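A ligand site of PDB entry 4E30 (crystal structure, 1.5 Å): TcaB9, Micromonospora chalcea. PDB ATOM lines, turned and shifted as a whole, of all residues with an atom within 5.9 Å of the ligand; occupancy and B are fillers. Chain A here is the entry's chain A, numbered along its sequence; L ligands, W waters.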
ATOM      1  N   ASP A  35       2.136  18.843   4.161  1.00  0.00           N
ATOM      2  CA  ASP A  35       2.938  18.614   2.952  1.00  0.00           C
ATOM      3  C   ASP A  35       4.148  19.558   2.961  1.00  0.00           C
ATOM      4  O   ASP A  35       4.771  19.704   1.884  1.00  0.00           O
ATOM      5  CB  ASP A  35       2.114  18.716   1.671  1.00  0.00           C
ATOM      6  CG  ASP A  35       1.581  17.360   1.230  1.00  0.00           C
ATOM      7  OD1 ASP A  35       2.309  16.361   1.388  1.00  0.00           O
ATOM      8  OD2 ASP A  35       0.443  17.271   0.732  1.00  0.00           O
ATOM      9  N   TYR A  80       2.809  17.127  -3.880  1.00  0.00           N
ATOM     10  CA  TYR A  80       2.113  15.847  -4.067  1.00  0.00           C
ATOM     11  C   TYR A  80       2.018  15.600  -5.565  1.00  0.00           C
ATOM     12  O   TYR A  80       1.543  16.441  -6.336  1.00  0.00           O
ATOM     13  CB  TYR A  80       0.663  15.946  -3.625  1.00  0.00           C
ATOM     14  CG  TYR A  80      -0.058  14.627  -3.767  1.00  0.00           C
ATOM     15  CD1 TYR A  80       0.363  13.518  -3.041  1.00  0.00           C
ATOM     16  CD2 TYR A  80      -1.165  14.487  -4.613  1.00  0.00           C
ATOM     17  CE1 TYR A  80      -0.272  12.283  -3.153  1.00  0.00           C
ATOM     18  CE2 TYR A  80      -1.800  13.252  -4.725  1.00  0.00           C
ATOM     19  CZ  TYR A  80      -1.345  12.168  -3.997  1.00  0.00           C
ATOM     20  OH  TYR A  80      -1.973  10.934  -4.046  1.00  0.00           O
ATOM     21  N   GLY A  84       2.509   9.335  -9.135  1.00  0.00           N
ATOM     22  CA  GLY A  84       3.419   8.414  -8.458  1.00  0.00           C
ATOM     23  C   GLY A  84       2.819   7.056  -8.150  1.00  0.00           C
ATOM     24  O   GLY A  84       3.543   6.146  -7.742  1.00  0.00           O
ATOM     25  N   SER A  85       1.523   6.859  -8.374  1.00  0.00           N
ATOM     26  CA  SER A  85       0.891   5.569  -8.118  1.00  0.00           C
ATOM     27  C   SER A  85       0.329   4.983  -9.424  1.00  0.00           C
ATOM     28  O   SER A  85      -0.460   5.639 -10.144  1.00  0.00           O
ATOM     29  CB  SER A  85      -0.331   5.769  -7.215  1.00  0.00           C
ATOM     30  OG  SER A  85      -1.194   4.644  -7.168  1.00  0.00           O
ATOM     31  N   SER A  86       0.750   3.750  -9.683  1.00  0.00           N
ATOM     32  CA  SER A  86       0.318   3.044 -10.905  1.00  0.00           C
ATOM     33  C   SER A  86      -1.172   2.729 -10.838  1.00  0.00           C
ATOM     34  O   SER A  86      -1.906   2.852 -11.815  1.00  0.00           O
ATOM     35  CB  SER A  86       1.139   1.783 -11.119  1.00  0.00           C
ATOM     36  OG  SER A  86       0.958   0.827 -10.066  1.00  0.00           O
ATOM     37  N   TYR A 224      -6.500  15.884   7.980  1.00  0.00           N
ATOM     38  CA  TYR A 224      -5.274  16.687   8.024  1.00  0.00           C
ATOM     39  C   TYR A 224      -5.656  17.979   7.317  1.00  0.00           C
ATOM     40  O   TYR A 224      -6.807  18.115   6.912  1.00  0.00           O
ATOM     41  CB  TYR A 224      -4.082  15.961   7.420  1.00  0.00           C
ATOM     42  CG  TYR A 224      -4.145  15.552   5.965  1.00  0.00           C
ATOM     43  CD1 TYR A 224      -3.667  16.395   4.954  1.00  0.00           C
ATOM     44  CD2 TYR A 224      -4.628  14.281   5.577  1.00  0.00           C
ATOM     45  CE1 TYR A 224      -3.665  16.036   3.604  1.00  0.00           C
ATOM     46  CE2 TYR A 224      -4.648  13.938   4.241  1.00  0.00           C
ATOM     47  CZ  TYR A 224      -4.212  14.824   3.254  1.00  0.00           C
ATOM     48  OH  TYR A 224      -4.189  14.484   1.915  1.00  0.00           O
ATOM     49  N   HIS A 227      -7.730  18.165   4.120  1.00  0.00           N
ATOM     50  CA  HIS A 227      -9.040  17.531   4.085  1.00  0.00           C
ATOM     51  C   HIS A 227     -10.018  18.181   5.072  1.00  0.00           C
ATOM     52  O   HIS A 227     -10.183  17.775   6.215  1.00  0.00           O
ATOM     53  CB  HIS A 227      -8.885  16.073   4.471  1.00  0.00           C
ATOM     54  CG  HIS A 227      -8.295  15.274   3.336  1.00  0.00           C
ATOM     55  ND1 HIS A 227      -8.019  13.926   3.430  1.00  0.00           N
ATOM     56  CD2 HIS A 227      -7.915  15.657   2.095  1.00  0.00           C
ATOM     57  CE1 HIS A 227      -7.505  13.501   2.290  1.00  0.00           C
ATOM     58  NE2 HIS A 227      -7.456  14.531   1.455  1.00  0.00           N
ATOM     59  N   HIS A 256      -7.662   5.188  -2.101  1.00  0.00           N
ATOM     60  CA  HIS A 256      -7.444   6.112  -1.001  1.00  0.00           C
ATOM     61  C   HIS A 256      -8.141   5.691   0.300  1.00  0.00           C
ATOM     62  O   HIS A 256      -8.627   6.591   1.027  1.00  0.00           O
ATOM     63  CB  HIS A 256      -7.748   7.548  -1.422  1.00  0.00           C
ATOM     64  CG  HIS A 256      -6.732   8.095  -2.375  1.00  0.00           C
ATOM     65  ND1 HIS A 256      -5.401   8.206  -2.032  1.00  0.00           N
ATOM     66  CD2 HIS A 256      -6.835   8.533  -3.641  1.00  0.00           C
ATOM     67  CE1 HIS A 256      -4.727   8.705  -3.052  1.00  0.00           C
ATOM     68  NE2 HIS A 256      -5.580   8.916  -4.051  1.00  0.00           N
ATOM     69  N   TYR A 325       7.109   3.768   5.743  1.00  0.00           N
ATOM     70  CA  TYR A 325       7.056   3.687   4.290  1.00  0.00           C
ATOM     71  C   TYR A 325       5.884   4.527   3.767  1.00  0.00           C
ATOM     72  O   TYR A 325       4.705   4.272   4.049  1.00  0.00           O
ATOM     73  CB  TYR A 325       6.876   2.237   3.877  1.00  0.00           C
ATOM     74  CG  TYR A 325       7.328   1.976   2.460  1.00  0.00           C
ATOM     75  CD1 TYR A 325       6.643   2.545   1.373  1.00  0.00           C
ATOM     76  CD2 TYR A 325       8.433   1.127   2.221  1.00  0.00           C
ATOM     77  CE1 TYR A 325       7.059   2.258   0.059  1.00  0.00           C
ATOM     78  CE2 TYR A 325       8.850   0.887   0.885  1.00  0.00           C
ATOM     79  CZ  TYR A 325       8.148   1.442  -0.181  1.00  0.00           C
ATOM     80  OH  TYR A 325       8.589   1.168  -1.462  1.00  0.00           O
ATOM     81  N   GLY A 326       6.289   5.529   2.988  1.00  0.00           N
ATOM     82  CA  GLY A 326       5.416   6.495   2.308  1.00  0.00           C
ATOM     83  C   GLY A 326       5.343   7.746   3.184  1.00  0.00           C
ATOM     84  O   GLY A 326       4.809   7.727   4.303  1.00  0.00           O
ATOM     85  N   ALA A 327       5.817   8.891   2.679  1.00  0.00           N
ATOM     86  CA  ALA A 327       5.758  10.175   3.415  1.00  0.00           C
ATOM     87  C   ALA A 327       4.464  10.857   2.986  1.00  0.00           C
ATOM     88  O   ALA A 327       4.411  11.908   2.335  1.00  0.00           O
ATOM     89  CB  ALA A 327       6.966  11.081   3.004  1.00  0.00           C
ATOM     90  N   THR A 328       3.396  10.167   3.355  1.00  0.00           N
ATOM     91  CA  THR A 328       2.063  10.647   3.026  1.00  0.00           C
ATOM     92  C   THR A 328       1.825  11.971   3.760  1.00  0.00           C
ATOM     93  O   THR A 328       2.374  12.185   4.833  1.00  0.00           O
ATOM     94  CB  THR A 328       1.006   9.654   3.549  1.00  0.00           C
ATOM     95  OG1 THR A 328       1.225   9.458   4.940  1.00  0.00           O
ATOM     96  CG2 THR A 328       1.125   8.267   2.806  1.00  0.00           C
ATOM     97  N   ALA A 329       0.979  12.859   3.238  1.00  0.00           N
ATOM     98  CA  ALA A 329       0.437  13.937   4.039  1.00  0.00           C
ATOM     99  C   ALA A 329      -0.291  13.441   5.298  1.00  0.00           C
ATOM    100  O   ALA A 329      -0.186  14.010   6.382  1.00  0.00           O
ATOM    101  CB  ALA A 329      -0.484  14.797   3.195  1.00  0.00           C
ATOM    102  N   LYS A 330      -1.033  12.340   5.094  1.00  0.00           N
ATOM    103  CA  LYS A 330      -1.753  11.722   6.205  1.00  0.00           C
ATOM    104  C   LYS A 330      -0.864  11.452   7.422  1.00  0.00           C
ATOM    105  O   LYS A 330      -1.289  11.546   8.579  1.00  0.00           O
ATOM    106  CB  LYS A 330      -2.350  10.392   5.735  1.00  0.00           C
ATOM    107  CG  LYS A 330      -3.497  10.584   4.703  1.00  0.00           C
ATOM    108  CD  LYS A 330      -4.225   9.246   4.397  1.00  0.00           C
ATOM    109  CE  LYS A 330      -3.331   8.127   3.801  1.00  0.00           C
ATOM    110  NZ  LYS A 330      -2.926   8.518   2.406  1.00  0.00           N
ATOM    111  N   SER A 331       0.344  11.012   7.091  1.00  0.00           N
ATOM    112  CA  SER A 331       1.248  10.600   8.165  1.00  0.00           C
ATOM    113  C   SER A 331       1.521  11.764   9.108  1.00  0.00           C
ATOM    114  O   SER A 331       1.827  11.531  10.275  1.00  0.00           O
ATOM    115  CB  SER A 331       2.531   9.961   7.664  1.00  0.00           C
ATOM    116  OG  SER A 331       3.420  10.877   7.021  1.00  0.00           O
ATOM    117  N   TYR A 349      10.631   6.105   3.877  1.00  0.00           N
ATOM    118  CA  TYR A 349      11.007   5.899   2.463  1.00  0.00           C
ATOM    119  C   TYR A 349       9.888   6.356   1.545  1.00  0.00           C
ATOM    120  O   TYR A 349       8.697   6.129   1.798  1.00  0.00           O
ATOM    121  CB  TYR A 349      11.404   4.413   2.267  1.00  0.00           C
ATOM    122  CG  TYR A 349      12.631   4.112   3.068  1.00  0.00           C
ATOM    123  CD1 TYR A 349      13.880   4.530   2.617  1.00  0.00           C
ATOM    124  CD2 TYR A 349      12.509   3.504   4.326  1.00  0.00           C
ATOM    125  CE1 TYR A 349      14.980   4.279   3.412  1.00  0.00           C
ATOM    126  CE2 TYR A 349      13.584   3.277   5.111  1.00  0.00           C
ATOM    127  CZ  TYR A 349      14.817   3.669   4.622  1.00  0.00           C
ATOM    128  OH  TYR A 349      15.919   3.440   5.423  1.00  0.00           O
ATOM    129  N   ASP A 350      10.258   7.119   0.510  1.00  0.00           N
ATOM    130  CA  ASP A 350       9.247   7.689  -0.370  1.00  0.00           C
ATOM    131  C   ASP A 350       9.724   7.903  -1.815  1.00  0.00           C
ATOM    132  O   ASP A 350      10.917   8.195  -1.999  1.00  0.00           O
ATOM    133  CB  ASP A 350       8.819   9.061   0.179  1.00  0.00           C
ATOM    134  CG  ASP A 350       7.556   9.581  -0.479  1.00  0.00           C
ATOM    135  OD1 ASP A 350       6.429   9.226  -0.029  1.00  0.00           O
ATOM    136  OD2 ASP A 350       7.665  10.382  -1.439  1.00  0.00           O
ATOM    137  N   THR A 351       8.834   7.752  -2.803  1.00  0.00           N
ATOM    138  CA  THR A 351       9.251   7.914  -4.197  1.00  0.00           C
ATOM    139  C   THR A 351       9.260   9.326  -4.738  1.00  0.00           C
ATOM    140  O   THR A 351       9.599   9.490  -5.918  1.00  0.00           O
ATOM    141  CB  THR A 351       8.407   7.015  -5.114  1.00  0.00           C
ATOM    142  OG1 THR A 351       7.038   7.246  -4.779  1.00  0.00           O
ATOM    143  CG2 THR A 351       8.747   5.563  -4.859  1.00  0.00           C
ATOM    144  N   THR A 352       8.901  10.338  -3.960  1.00  0.00           N
ATOM    145  CA  THR A 352       8.704  11.704  -4.438  1.00  0.00           C
ATOM    146  C   THR A 352      10.025  12.459  -4.292  1.00  0.00           C
ATOM    147  O   THR A 352      10.450  12.754  -3.177  1.00  0.00           O
ATOM    148  CB  THR A 352       7.577  12.466  -3.693  1.00  0.00           C
ATOM    149  OG1 THR A 352       6.416  11.613  -3.504  1.00  0.00           O
ATOM    150  CG2 THR A 352       7.119  13.720  -4.449  1.00  0.00           C
ATOM    151  N   LYS A 355      10.289  15.303  -1.835  1.00  0.00           N
ATOM    152  CA  LYS A 355      10.166  15.018  -0.398  1.00  0.00           C
ATOM    153  C   LYS A 355      11.436  14.354   0.105  1.00  0.00           C
ATOM    154  O   LYS A 355      11.710  14.317   1.295  1.00  0.00           O
ATOM    155  CB  LYS A 355       9.034  14.007  -0.147  1.00  0.00           C
ATOM    156  CG  LYS A 355       7.648  14.652  -0.471  1.00  0.00           C
ATOM    157  CD  LYS A 355       6.571  13.541  -0.156  1.00  0.00           C
ATOM    158  CE  LYS A 355       5.195  14.035  -0.560  1.00  0.00           C
ATOM    159  NZ  LYS A 355       4.099  13.063  -0.175  1.00  0.00           N
ATOM    160  N   ALA A 370      12.839   5.633  -1.904  1.00  0.00           N
ATOM    161  CA  ALA A 370      12.394   4.250  -1.705  1.00  0.00           C
ATOM    162  C   ALA A 370      13.467   3.288  -2.187  1.00  0.00           C
ATOM    163  O   ALA A 370      13.596   2.177  -1.674  1.00  0.00           O
ATOM    164  CB  ALA A 370      11.103   4.035  -2.508  1.00  0.00           C
ATOM    165  N   PHE A 384       2.715   3.893   6.337  1.00  0.00           N
ATOM    166  CA  PHE A 384       1.905   5.103   6.293  1.00  0.00           C
ATOM    167  C   PHE A 384       1.100   5.098   5.008  1.00  0.00           C
ATOM    168  O   PHE A 384      -0.041   5.567   5.063  1.00  0.00           O
ATOM    169  CB  PHE A 384       2.826   6.328   6.276  1.00  0.00           C
ATOM    170  CG  PHE A 384       3.477   6.595   7.609  1.00  0.00           C
ATOM    171  CD1 PHE A 384       2.766   6.657   8.779  1.00  0.00           C
ATOM    172  CD2 PHE A 384       4.851   6.825   7.642  1.00  0.00           C
ATOM    173  CE1 PHE A 384       3.380   6.931  10.008  1.00  0.00           C
ATOM    174  CE2 PHE A 384       5.495   7.120   8.841  1.00  0.00           C
ATOM    175  CZ  PHE A 384       4.769   7.177  10.031  1.00  0.00           C
ATOM    176  N   ALA A 385       1.693   4.673   3.884  1.00  0.00           N
ATOM    177  CA  ALA A 385       0.912   4.587   2.632  1.00  0.00           C
ATOM    178  C   ALA A 385       0.058   3.323   2.608  1.00  0.00           C
ATOM    179  O   ALA A 385       0.094   2.574   1.624  1.00  0.00           O
ATOM    180  CB  ALA A 385       1.870   4.776   1.424  1.00  0.00           C
ATOM    181  N   ASN A 387      -3.039   2.942   2.163  1.00  0.00           N
ATOM    182  CA  ASN A 387      -4.002   2.941   1.033  1.00  0.00           C
ATOM    183  C   ASN A 387      -3.413   2.458  -0.287  1.00  0.00           C
ATOM    184  O   ASN A 387      -4.146   2.143  -1.239  1.00  0.00           O
ATOM    185  CB  ASN A 387      -4.571   4.354   0.856  1.00  0.00           C
ATOM    186  CG  ASN A 387      -3.503   5.442   0.795  1.00  0.00           C
ATOM    187  OD1 ASN A 387      -2.703   5.599   1.732  1.00  0.00           O
ATOM    188  ND2 ASN A 387      -3.515   6.233  -0.270  1.00  0.00           N
ATOM    189  N   HIS A 388      -2.086   2.377  -0.309  1.00  0.00           N
ATOM    190  CA  HIS A 388      -1.315   1.857  -1.449  1.00  0.00           C
ATOM    191  C   HIS A 388      -0.683   0.506  -1.107  1.00  0.00           C
ATOM    192  O   HIS A 388       0.309   0.107  -1.740  1.00  0.00           O
ATOM    193  CB  HIS A 388      -0.180   2.833  -1.775  1.00  0.00           C
ATOM    194  CG  HIS A 388      -0.675   4.160  -2.283  1.00  0.00           C
ATOM    195  ND1 HIS A 388      -1.364   4.257  -3.474  1.00  0.00           N
ATOM    196  CD2 HIS A 388      -0.659   5.413  -1.754  1.00  0.00           C
ATOM    197  CE1 HIS A 388      -1.694   5.518  -3.694  1.00  0.00           C
ATOM    198  NE2 HIS A 388      -1.282   6.234  -2.655  1.00  0.00           N
ATOM    199  N   GLU A 391       0.023  -2.158  -4.100  1.00  0.00           N
ATOM    200  CA  GLU A 391       1.007  -1.672  -5.077  1.00  0.00           C
ATOM    201  C   GLU A 391       2.411  -1.648  -4.470  1.00  0.00           C
ATOM    202  O   GLU A 391       3.403  -2.035  -5.095  1.00  0.00           O
ATOM    203  CB  GLU A 391       0.584  -0.256  -5.486  1.00  0.00           C
ATOM    204  CG  GLU A 391       1.567   0.382  -6.424  1.00  0.00           C
ATOM    205  CD  GLU A 391       1.122   1.706  -7.016  1.00  0.00           C
ATOM    206  OE1 GLU A 391       2.013   2.368  -7.581  1.00  0.00           O
ATOM    207  OE2 GLU A 391      -0.076   2.012  -6.893  1.00  0.00           O
ATOM    208  N   ILE A 392       2.494  -1.198  -3.218  1.00  0.00           N
ATOM    209  CA  ILE A 392       3.781  -1.079  -2.541  1.00  0.00           C
ATOM    210  C   ILE A 392       4.324  -2.465  -2.188  1.00  0.00           C
ATOM    211  O   ILE A 392       5.492  -2.760  -2.444  1.00  0.00           O
ATOM    212  CB  ILE A 392       3.710  -0.225  -1.253  1.00  0.00           C
ATOM    213  CG1 ILE A 392       3.759   1.246  -1.664  1.00  0.00           C
ATOM    214  CG2 ILE A 392       5.035  -0.444  -0.472  1.00  0.00           C
ATOM    215  CD1 ILE A 392       3.372   2.197  -0.523  1.00  0.00           C
ATOM    216  N   LYS A 395       5.995  -4.341  -4.904  1.00  0.00           N
ATOM    217  CA  LYS A 395       7.306  -3.820  -5.302  1.00  0.00           C
ATOM    218  C   LYS A 395       8.329  -4.214  -4.240  1.00  0.00           C
ATOM    219  O   LYS A 395       9.521  -4.048  -4.489  1.00  0.00           O
ATOM    220  CB  LYS A 395       7.310  -2.300  -5.441  1.00  0.00           C
ATOM    221  CG  LYS A 395       6.541  -1.803  -6.654  1.00  0.00           C
ATOM    222  CD  LYS A 395       6.898  -0.380  -6.993  1.00  0.00           C
ATOM    223  CE  LYS A 395       6.074   0.505  -6.101  1.00  0.00           C
ATOM    224  NZ  LYS A 395       6.439   1.907  -6.486  1.00  0.00           N
HETATM  225  P1  LIG L   1      -0.988   9.241  -0.834  1.00  0.00           P
HETATM  226  O1  LIG L   1      -1.493   8.144   0.061  1.00  0.00           O
HETATM  227  O2  LIG L   1      -1.304   9.098  -2.305  1.00  0.00           O
HETATM  228  O3  LIG L   1      -1.526  10.719  -0.476  1.00  0.00           O
HETATM  229  P2  LIG L   1      -1.565  11.672   0.817  1.00  0.00           P
HETATM  230  O4  LIG L   1      -1.627  10.855   2.061  1.00  0.00           O
HETATM  231  O5  LIG L   1      -0.390  12.630   0.764  1.00  0.00           O
HETATM  232  O6  LIG L   1      -2.930  12.309   0.582  1.00  0.00           O
HETATM  233  O7  LIG L   1       0.604   9.365  -0.682  1.00  0.00           O
HETATM  234  C1  LIG L   1       1.459   8.286  -0.993  1.00  0.00           C
HETATM  235  C2  LIG L   1       2.883   8.719  -0.661  1.00  0.00           C
HETATM  236  O8  LIG L   1       3.539   7.436  -0.705  1.00  0.00           O
HETATM  237  C3  LIG L   1       3.463   9.596  -1.784  1.00  0.00           C
HETATM  238  O9  LIG L   1       4.430  10.498  -1.177  1.00  0.00           O
HETATM  239  C4  LIG L   1       4.174   8.530  -2.595  1.00  0.00           C
HETATM  240  C5  LIG L   1       4.599   7.407  -1.667  1.00  0.00           C
HETATM  241  N1  LIG L   1       4.520   6.154  -2.416  1.00  0.00           N
HETATM  242  C6  LIG L   1       5.690   5.375  -2.449  1.00  0.00           C
HETATM  243  O10 LIG L   1       6.709   5.760  -1.853  1.00  0.00           O
HETATM  244  N2  LIG L   1       5.664   4.211  -3.114  1.00  0.00           N
HETATM  245  C7  LIG L   1       4.620   3.758  -3.815  1.00  0.00           C
HETATM  246  O11 LIG L   1       4.678   2.658  -4.404  1.00  0.00           O
HETATM  247  C8  LIG L   1       3.361   4.551  -3.792  1.00  0.00           C
HETATM  248  C9  LIG L   1       2.077   4.181  -4.486  1.00  0.00           C
HETATM  249  C10 LIG L   1       3.404   5.735  -3.056  1.00  0.00           C
HETATM  250  O   HOH W   1       5.786   5.568  -6.470  1.00  0.00           O
HETATM  251  O   HOH W   2       2.833  10.225  -5.231  1.00  0.00           O
HETATM  252  O   HOH W   3       0.674   8.503  -4.577  1.00  0.00           O
HETATM  253  O   HOH W   4       7.894   2.499  -3.596  1.00  0.00           O
HETATM  254  O   HOH W   5      -1.479  15.280  -0.041  1.00  0.00           O
HETATM  255  O   HOH W   6       3.683  12.672  -3.760  1.00  0.00           O
HETATM  256  O   HOH W   7      -4.469  12.909  -1.369  1.00  0.00           O
HETATM  257  O   HOH W   8       1.647  14.203  -0.027  1.00  0.00           O
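OH of Tyr 80 is in hydrogen-bond range of O2 of the ligand (2.6 Å). The side-chain carboxylate (OD1) of Asp 350 lies within hydrogen-bond range of an oxygen (O9) of the ligand (2.6 Å). N of Lys 330 sits close to O4 of the ligand (3.4 Å). The side-chain amino group (NZ) of Lys 330 is in salt-bridge range of an oxygen (O4) of the ligand, 2.7 Å away. An oxygen (O9) of the ligand is in hydrogen-bond range of the side-chain amino group (NZ) of Lys 355. An oxygen (O1) of the ligand lies within hydrogen-bond range of the side-chain amide nitrogen (ND2) of Asn 387 (2.8 Å). NZ of Lys 395 sits at hydrogen-bond distance from O11 of the ligand (2.8 Å). The backbone NH (N) of Ala 329 is in hydrogen-bond range of an oxygen (O5) of the ligand. An oxygen (O6) of the ligand lies within hydrogen-bond range of the side-chain hydroxyl (OH) of Tyr 224 (2.8 Å). O2 of the ligand is in hydrogen-bond range of NE2 of His 388, 2.9 Å away. O10 of the ligand is in hydrogen-bond range of N of Thr 351, at 3.1 Å. An oxygen (O10) of the ligand lies close to the side-chain hydroxyl (OG1) of Thr 351 (3.3 Å). The side-chain hydroxyl (OG1) of Thr 352 lies within hydrogen-bond range of an oxygen (O9) of the ligand, at 3.3 Å.
Water W8 lies within hydrogen-bond range of OD1 of Asp 35, O5 of the ligand and NZ of Lys 355. Water W4 lies within hydrogen-bond range of the side-chain hydroxyl (OH) of Tyr 325 (2.6 Å), a nitrogen (N2) of the ligand (2.9 Å) and the side-chain amino group (NZ) of Lys 395 (3.3 Å). Water W5 lies within hydrogen-bond range of the side-chain carboxylate of Asp 35 (2.9 Å), an oxygen (O5) of the ligand (3.0 Å) and the side-chain hydroxyl of Tyr 224 (3.4 Å). Water W1 bridges the backbone carbonyl oxygen (O) of Gly 84 (2.6 Å) and the side-chain hydroxyl (OG1) of Thr 351 (2.7 Å). Water W6 bridges OG1 of Thr 352 (2.9 Å) and O9 of the ligand (3.5 Å).
OG1 of Thr 352 is in hydrogen-bond range of OD2 of Asp 350 (2.7 Å). OD1 of Asp 350 lies within hydrogen-bond range of N of Ala 327 (2.8 Å). The backbone carbonyl oxygen of Asp 350 is in hydrogen-bond range of the backbone NH of Ala 370 (3.2 Å). The side-chain amino group (NZ) of Lys 355 sits at hydrogen-bond distance from the backbone carbonyl oxygen (O) of Ala 327, 2.8 Å away. ND2 of Asn 387 sits at hydrogen-bond distance from NE2 of His 388, 3.3 Å away. OH of Tyr 224 lies within hydrogen-bond range of NE2 of His 227, at 3.3 Å. The side-chain carboxylate of Glu 391 is in hydrogen-bond range of the backbone NH of Ser 86, 2.8 Å away. The backbone carbonyl oxygen (O) of Tyr 325 sits at hydrogen-bond distance from the backbone NH (N) of Phe 384 (3.1 Å).
Residues that only touch the ligand: Ser 85 (3.97 Å), His 256 (3.5 Å), Tyr 325 (3.98 Å), Gly 326 (3.7 Å), Ala 327 (3.8 Å), Thr 328 (3.3 Å), Ala 385 (3.8 Å), Glu 391 (3.6 Å) and Ile 392 (3.2 Å). Within 4 Å of the ligand: Tyr 80, Ser 85, Tyr 224, His 256, Tyr 325, Gly 326, Ala 327, Thr 328, Ala 329, Lys 330, Asp 350, Thr 351, Thr 352, Lys 355, Ala 385, Asn 387, His 388, Glu 391, Ile 392 and Lys 395.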
